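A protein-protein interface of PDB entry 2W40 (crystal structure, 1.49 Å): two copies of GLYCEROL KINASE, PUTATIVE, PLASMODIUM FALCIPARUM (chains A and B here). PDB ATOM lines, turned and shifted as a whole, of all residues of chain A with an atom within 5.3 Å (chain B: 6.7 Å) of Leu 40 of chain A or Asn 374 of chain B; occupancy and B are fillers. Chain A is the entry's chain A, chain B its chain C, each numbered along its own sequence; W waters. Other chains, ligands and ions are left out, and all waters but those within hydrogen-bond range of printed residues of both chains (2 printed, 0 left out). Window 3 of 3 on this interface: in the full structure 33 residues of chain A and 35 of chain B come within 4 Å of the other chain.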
ATOM      1  N   LYS A  38      12.245 -28.426 -19.087  1.00  0.00           N
ATOM      2  CA  LYS A  38      11.825 -27.402 -20.022  1.00  0.00           C
ATOM      3  C   LYS A  38      10.831 -27.982 -21.028  1.00  0.00           C
ATOM      4  O   LYS A  38      11.159 -28.811 -21.890  1.00  0.00           O
ATOM      5  CB  LYS A  38      13.025 -26.800 -20.739  1.00  0.00           C
ATOM      6  CG  LYS A  38      14.160 -26.288 -19.828  1.00  0.00           C
ATOM      7  CD  LYS A  38      15.353 -25.981 -20.713  1.00  0.00           C
ATOM      8  CE  LYS A  38      16.483 -25.456 -19.881  1.00  0.00           C
ATOM      9  NZ  LYS A  38      16.611 -23.964 -19.796  1.00  0.00           N
ATOM     10  N   CYS A  39       9.592 -27.503 -20.938  1.00  0.00           N
ATOM     11  CA  CYS A  39       8.526 -27.937 -21.822  1.00  0.00           C
ATOM     12  C   CYS A  39       7.872 -26.700 -22.478  1.00  0.00           C
ATOM     13  O   CYS A  39       6.748 -26.335 -22.123  1.00  0.00           O
ATOM     14  CB  CYS A  39       7.502 -28.754 -21.085  1.00  0.00           C
ATOM     15  SG  CYS A  39       8.153 -30.178 -20.235  1.00  0.00           S
ATOM     16  N   LEU A  40       8.615 -26.121 -23.404  1.00  0.00           N
ATOM     17  CA  LEU A  40       8.336 -24.813 -24.075  1.00  0.00           C
ATOM     18  C   LEU A  40       7.243 -24.795 -25.026  1.00  0.00           C
ATOM     19  O   LEU A  40       6.636 -23.739 -25.212  1.00  0.00           O
ATOM     20  CB  LEU A  40       9.619 -24.407 -24.849  1.00  0.00           C
ATOM     21  CG  LEU A  40       9.859 -23.146 -25.728  1.00  0.00           C
ATOM     22  CD1 LEU A  40       9.861 -21.928 -24.794  1.00  0.00           C
ATOM     23  CD2 LEU A  40      11.176 -23.209 -26.622  1.00  0.00           C
ATOM     24  N   LYS A  41       6.990 -25.911 -25.703  1.00  0.00           N
ATOM     25  CA  LYS A  41       6.024 -26.030 -26.730  1.00  0.00           C
ATOM     26  C   LYS A  41       5.414 -27.419 -26.496  1.00  0.00           C
ATOM     27  O   LYS A  41       6.102 -28.332 -25.961  1.00  0.00           O
ATOM     28  CB  LYS A  41       6.653 -25.987 -28.171  1.00  0.00           C
ATOM     29  CG  LYS A  41       7.646 -24.903 -28.416  1.00  0.00           C
ATOM     30  CD  LYS A  41       8.083 -25.067 -29.862  1.00  0.00           C
ATOM     31  CE  LYS A  41       9.028 -24.023 -30.225  1.00  0.00           C
ATOM     32  NZ  LYS A  41       8.971 -23.947 -31.711  1.00  0.00           N
ATOM     33  N   PRO A  42       4.179 -27.660 -27.010  1.00  0.00           N
ATOM     34  CA  PRO A  42       3.637 -29.024 -26.981  1.00  0.00           C
ATOM     35  C   PRO A  42       4.578 -30.027 -27.626  1.00  0.00           C
ATOM     36  O   PRO A  42       5.017 -29.867 -28.800  1.00  0.00           O
ATOM     37  CB  PRO A  42       2.316 -28.912 -27.761  1.00  0.00           C
ATOM     38  CG  PRO A  42       1.932 -27.425 -27.674  1.00  0.00           C
ATOM     39  CD  PRO A  42       3.253 -26.733 -27.740  1.00  0.00           C
ATOM     40  N   GLY A  43       4.909 -31.094 -26.882  1.00  0.00           N
ATOM     41  CA  GLY A  43       5.821 -32.077 -27.446  1.00  0.00           C
ATOM     42  C   GLY A  43       7.248 -31.925 -27.080  1.00  0.00           C
ATOM     43  O   GLY A  43       7.993 -32.860 -27.119  1.00  0.00           O
ATOM     44  N   TRP A  44       7.661 -30.722 -26.806  1.00  0.00           N
ATOM     45  CA  TRP A  44       9.084 -30.431 -26.511  1.00  0.00           C
ATOM     46  C   TRP A  44       9.403 -30.749 -25.038  1.00  0.00           C
ATOM     47  O   TRP A  44       8.653 -30.360 -24.079  1.00  0.00           O
ATOM     48  CB  TRP A  44       9.412 -28.964 -26.795  1.00  0.00           C
ATOM     49  CG  TRP A  44       9.492 -28.686 -28.254  1.00  0.00           C
ATOM     50  CD1 TRP A  44       8.724 -29.213 -29.243  1.00  0.00           C
ATOM     51  CD2 TRP A  44      10.421 -27.805 -28.889  1.00  0.00           C
ATOM     52  NE1 TRP A  44       9.121 -28.715 -30.499  1.00  0.00           N
ATOM     53  CE2 TRP A  44      10.149 -27.829 -30.290  1.00  0.00           C
ATOM     54  CE3 TRP A  44      11.409 -26.954 -28.412  1.00  0.00           C
ATOM     55  CZ2 TRP A  44      10.908 -27.116 -31.200  1.00  0.00           C
ATOM     56  CZ3 TRP A  44      12.129 -26.194 -29.344  1.00  0.00           C
ATOM     57  CH2 TRP A  44      11.860 -26.308 -30.712  1.00  0.00           C
ATOM     58  N   LYS A 323       2.369 -29.072 -10.633  1.00  0.00           N
ATOM     59  CA  LYS A 323       2.559 -27.770 -11.333  1.00  0.00           C
ATOM     60  C   LYS A 323       1.216 -27.066 -11.547  1.00  0.00           C
ATOM     61  O   LYS A 323       1.105 -25.836 -11.388  1.00  0.00           O
ATOM     62  CB  LYS A 323       3.226 -27.987 -12.674  1.00  0.00           C
ATOM     63  CG  LYS A 323       3.464 -26.737 -13.509  1.00  0.00           C
ATOM     64  CD  LYS A 323       3.837 -27.003 -15.036  1.00  0.00           C
ATOM     65  CE  LYS A 323       2.562 -27.377 -15.862  1.00  0.00           C
ATOM     66  NZ  LYS A 323       2.516 -27.692 -17.239  1.00  0.00           N
ATOM     67  N   THR B 344      -3.524 -24.713 -27.202  1.00  0.00           N
ATOM     68  CA  THR B 344      -2.624 -25.710 -27.823  1.00  0.00           C
ATOM     69  C   THR B 344      -3.320 -27.046 -28.153  1.00  0.00           C
ATOM     70  O   THR B 344      -2.737 -28.169 -28.013  1.00  0.00           O
ATOM     71  CB  THR B 344      -1.433 -25.930 -26.982  1.00  0.00           C
ATOM     72  OG1 THR B 344      -1.807 -26.735 -25.908  1.00  0.00           O
ATOM     73  CG2 THR B 344      -0.893 -24.655 -26.404  1.00  0.00           C
ATOM     74  N   MET B 371      -4.062 -32.874 -24.056  1.00  0.00           N
ATOM     75  CA  MET B 371      -3.011 -32.338 -23.161  1.00  0.00           C
ATOM     76  C   MET B 371      -1.624 -32.962 -23.398  1.00  0.00           C
ATOM     77  O   MET B 371      -1.459 -34.154 -23.700  1.00  0.00           O
ATOM     78  CB  MET B 371      -3.432 -32.483 -21.696  1.00  0.00           C
ATOM     79  CG  MET B 371      -4.817 -31.940 -21.343  1.00  0.00           C
ATOM     80  SD  MET B 371      -5.134 -31.894 -19.607  1.00  0.00           S
ATOM     81  CE  MET B 371      -5.374 -33.650 -19.243  1.00  0.00           C
ATOM     82  N   THR B 372      -0.639 -32.082 -23.253  1.00  0.00           N
ATOM     83  CA  THR B 372       0.742 -32.409 -23.233  1.00  0.00           C
ATOM     84  C   THR B 372       1.419 -31.900 -21.955  1.00  0.00           C
ATOM     85  O   THR B 372       0.792 -31.182 -21.144  1.00  0.00           O
ATOM     86  CB  THR B 372       1.468 -31.851 -24.513  1.00  0.00           C
ATOM     87  OG1 THR B 372       1.413 -30.419 -24.555  1.00  0.00           O
ATOM     88  CG2 THR B 372       0.877 -32.533 -25.835  1.00  0.00           C
ATOM     89  N   PHE B 373       2.739 -32.194 -21.807  1.00  0.00           N
ATOM     90  CA  PHE B 373       3.458 -31.657 -20.652  1.00  0.00           C
ATOM     91  C   PHE B 373       3.521 -30.098 -20.647  1.00  0.00           C
ATOM     92  O   PHE B 373       3.645 -29.455 -19.582  1.00  0.00           O
ATOM     93  CB  PHE B 373       4.814 -32.247 -20.486  1.00  0.00           C
ATOM     94  CG  PHE B 373       4.832 -33.645 -19.985  1.00  0.00           C
ATOM     95  CD1 PHE B 373       4.261 -33.987 -18.797  1.00  0.00           C
ATOM     96  CD2 PHE B 373       5.450 -34.629 -20.753  1.00  0.00           C
ATOM     97  CE1 PHE B 373       4.282 -35.352 -18.339  1.00  0.00           C
ATOM     98  CE2 PHE B 373       5.468 -35.951 -20.287  1.00  0.00           C
ATOM     99  CZ  PHE B 373       4.940 -36.295 -19.098  1.00  0.00           C
ATOM    100  N   ASN B 374       3.431 -29.516 -21.843  1.00  0.00           N
ATOM    101  CA  ASN B 374       3.374 -28.049 -21.999  1.00  0.00           C
ATOM    102  C   ASN B 374       2.061 -27.409 -21.486  1.00  0.00           C
ATOM    103  O   ASN B 374       2.018 -26.215 -21.153  1.00  0.00           O
ATOM    104  CB  ASN B 374       3.634 -27.720 -23.455  1.00  0.00           C
ATOM    105  CG  ASN B 374       3.473 -26.222 -23.770  1.00  0.00           C
ATOM    106  OD1 ASN B 374       2.446 -25.855 -24.339  1.00  0.00           O
ATOM    107  ND2 ASN B 374       4.424 -25.356 -23.294  1.00  0.00           N
ATOM    108  N   THR B 375       0.973 -28.229 -21.444  1.00  0.00           N
ATOM    109  CA  THR B 375      -0.363 -27.734 -21.031  1.00  0.00           C
ATOM    110  C   THR B 375      -0.309 -27.292 -19.579  1.00  0.00           C
ATOM    111  O   THR B 375       0.214 -27.974 -18.726  1.00  0.00           O
ATOM    112  CB  THR B 375      -1.431 -28.824 -21.214  1.00  0.00           C
ATOM    113  OG1 THR B 375      -1.354 -29.298 -22.574  1.00  0.00           O
ATOM    114  CG2 THR B 375      -2.873 -28.329 -20.781  1.00  0.00           C
ATOM    115  N   GLU B 376      -0.918 -26.122 -19.327  1.00  0.00           N
ATOM    116  CA  GLU B 376      -0.995 -25.496 -18.039  1.00  0.00           C
ATOM    117  C   GLU B 376      -2.441 -25.271 -17.679  1.00  0.00           C
ATOM    118  O   GLU B 376      -3.351 -25.374 -18.510  1.00  0.00           O
ATOM    119  CB  GLU B 376      -0.378 -24.080 -18.057  1.00  0.00           C
ATOM    120  CG  GLU B 376       1.006 -24.041 -18.558  1.00  0.00           C
ATOM    121  CD  GLU B 376       1.790 -22.931 -17.971  1.00  0.00           C
ATOM    122  OE1 GLU B 376       1.219 -22.056 -17.233  1.00  0.00           O
ATOM    123  OE2 GLU B 376       2.988 -22.952 -18.249  1.00  0.00           O
ATOM    124  N   HIS B 379      -4.488 -23.085 -20.053  1.00  0.00           N
ATOM    125  CA  HIS B 379      -5.021 -23.649 -21.267  1.00  0.00           C
ATOM    126  C   HIS B 379      -6.304 -24.429 -21.015  1.00  0.00           C
ATOM    127  O   HIS B 379      -7.231 -24.428 -21.834  1.00  0.00           O
ATOM    128  CB  HIS B 379      -4.013 -24.606 -21.938  1.00  0.00           C
ATOM    129  CG  HIS B 379      -2.662 -24.036 -22.179  1.00  0.00           C
ATOM    130  ND1 HIS B 379      -2.373 -23.145 -23.203  1.00  0.00           N
ATOM    131  CD2 HIS B 379      -1.485 -24.338 -21.612  1.00  0.00           C
ATOM    132  CE1 HIS B 379      -1.066 -22.908 -23.223  1.00  0.00           C
ATOM    133  NE2 HIS B 379      -0.511 -23.617 -22.260  1.00  0.00           N
HETATM  134  O   HOH W   1       5.324 -29.130 -17.401  1.00  0.00           O
HETATM  135  O   HOH W   2       4.171 -22.547 -23.036  1.00  0.00           O
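The backbone carbonyl oxygen (O) of Cys 39 of chain A lies within hydrogen-bond range of the side-chain amide nitrogen (ND2) of Asn 374 of chain B (2.8 Å).
The side-chain amino group (NZ) of Lys 323 of chain A is in hydrogen-bond range of the backbone carbonyl oxygen (O) of Phe 373 of chain B (3.1 Å).
The side-chain amino group (NZ) of Lys 323 of chain A sits at hydrogen-bond distance from the backbone carbonyl oxygen (O) of Thr 375 of chain B (2.8 Å).
The backbone carbonyl oxygen (O) of Leu 40 of chain A sits at hydrogen-bond distance from the side-chain amide nitrogen (ND2) of Asn 374 of chain B (3.3 Å).
The side-chain hydroxyl of Thr 372 of chain B lies close to the backbone NH of Asn 374 of chain B (3.5 Å).
The side-chain hydroxyl (OG1) of Thr 375 of chain B is in hydrogen-bond range of the backbone NH (N) of Thr 372 of chain B (3.0 Å).
CB of Phe 373 of chain B touches SG of Cys 39 of chain A, 3.9 Å away.
CB of Asn 374 of chain B touches C of Lys 41 of chain A (3.5 Å).
CB of Thr 344 of chain B touches CG of Pro 42 of chain A, 3.7 Å away.
Thr 372 of chain B touches Pro 42 of chain A.
N of Pro 42 of chain A touches CB of Asn 374 of chain B (3.6 Å).
Lys 38 of chain A touches none of the printed residues of chain B.
Printed residues of chain B within 4 Å of Cys 39 of chain A: Phe 373 and Asn 374.
Of the printed residues of chain B, Pro 42 of chain A touches Thr 344, Thr 372 and Asn 374.
Asn 374 of chain B touches four residues of chain A.
Printed residues of chain A within 4 Å of Thr 375 of chain B: Lys 323 (2.8 Å).
The nearest printed residue of chain B that does not touch Leu 40 of chain A is Phe 373 of chain B (7.0 Å).
The nearest residue of chain A that does not touch Asn 374 of chain B is Lys 323 of chain A (4.2 Å).
The nearest printed residue of chain B that does not touch Cys 39 of chain A is Thr 375 of chain B (6.1 Å).
Hydrophobic or aromatic side chains of chain A that line the printed part of chain B: Pro 42.
Among the printed residues, 9 pairs touch across the chains.
Among the printed residues, no Asp or Glu carboxylate lies within 4 Å of a Lys or Arg side-chain nitrogen of the other chain.
No position is printed for both chains.
Water W1 bridges O of Phe 373 of chain B and NZ of Lys 323 of chain A.
Water W2 bridges ND2 of Asn 374 of chain B (2.8 Å) and O of Leu 40 of chain A (3.5 Å).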
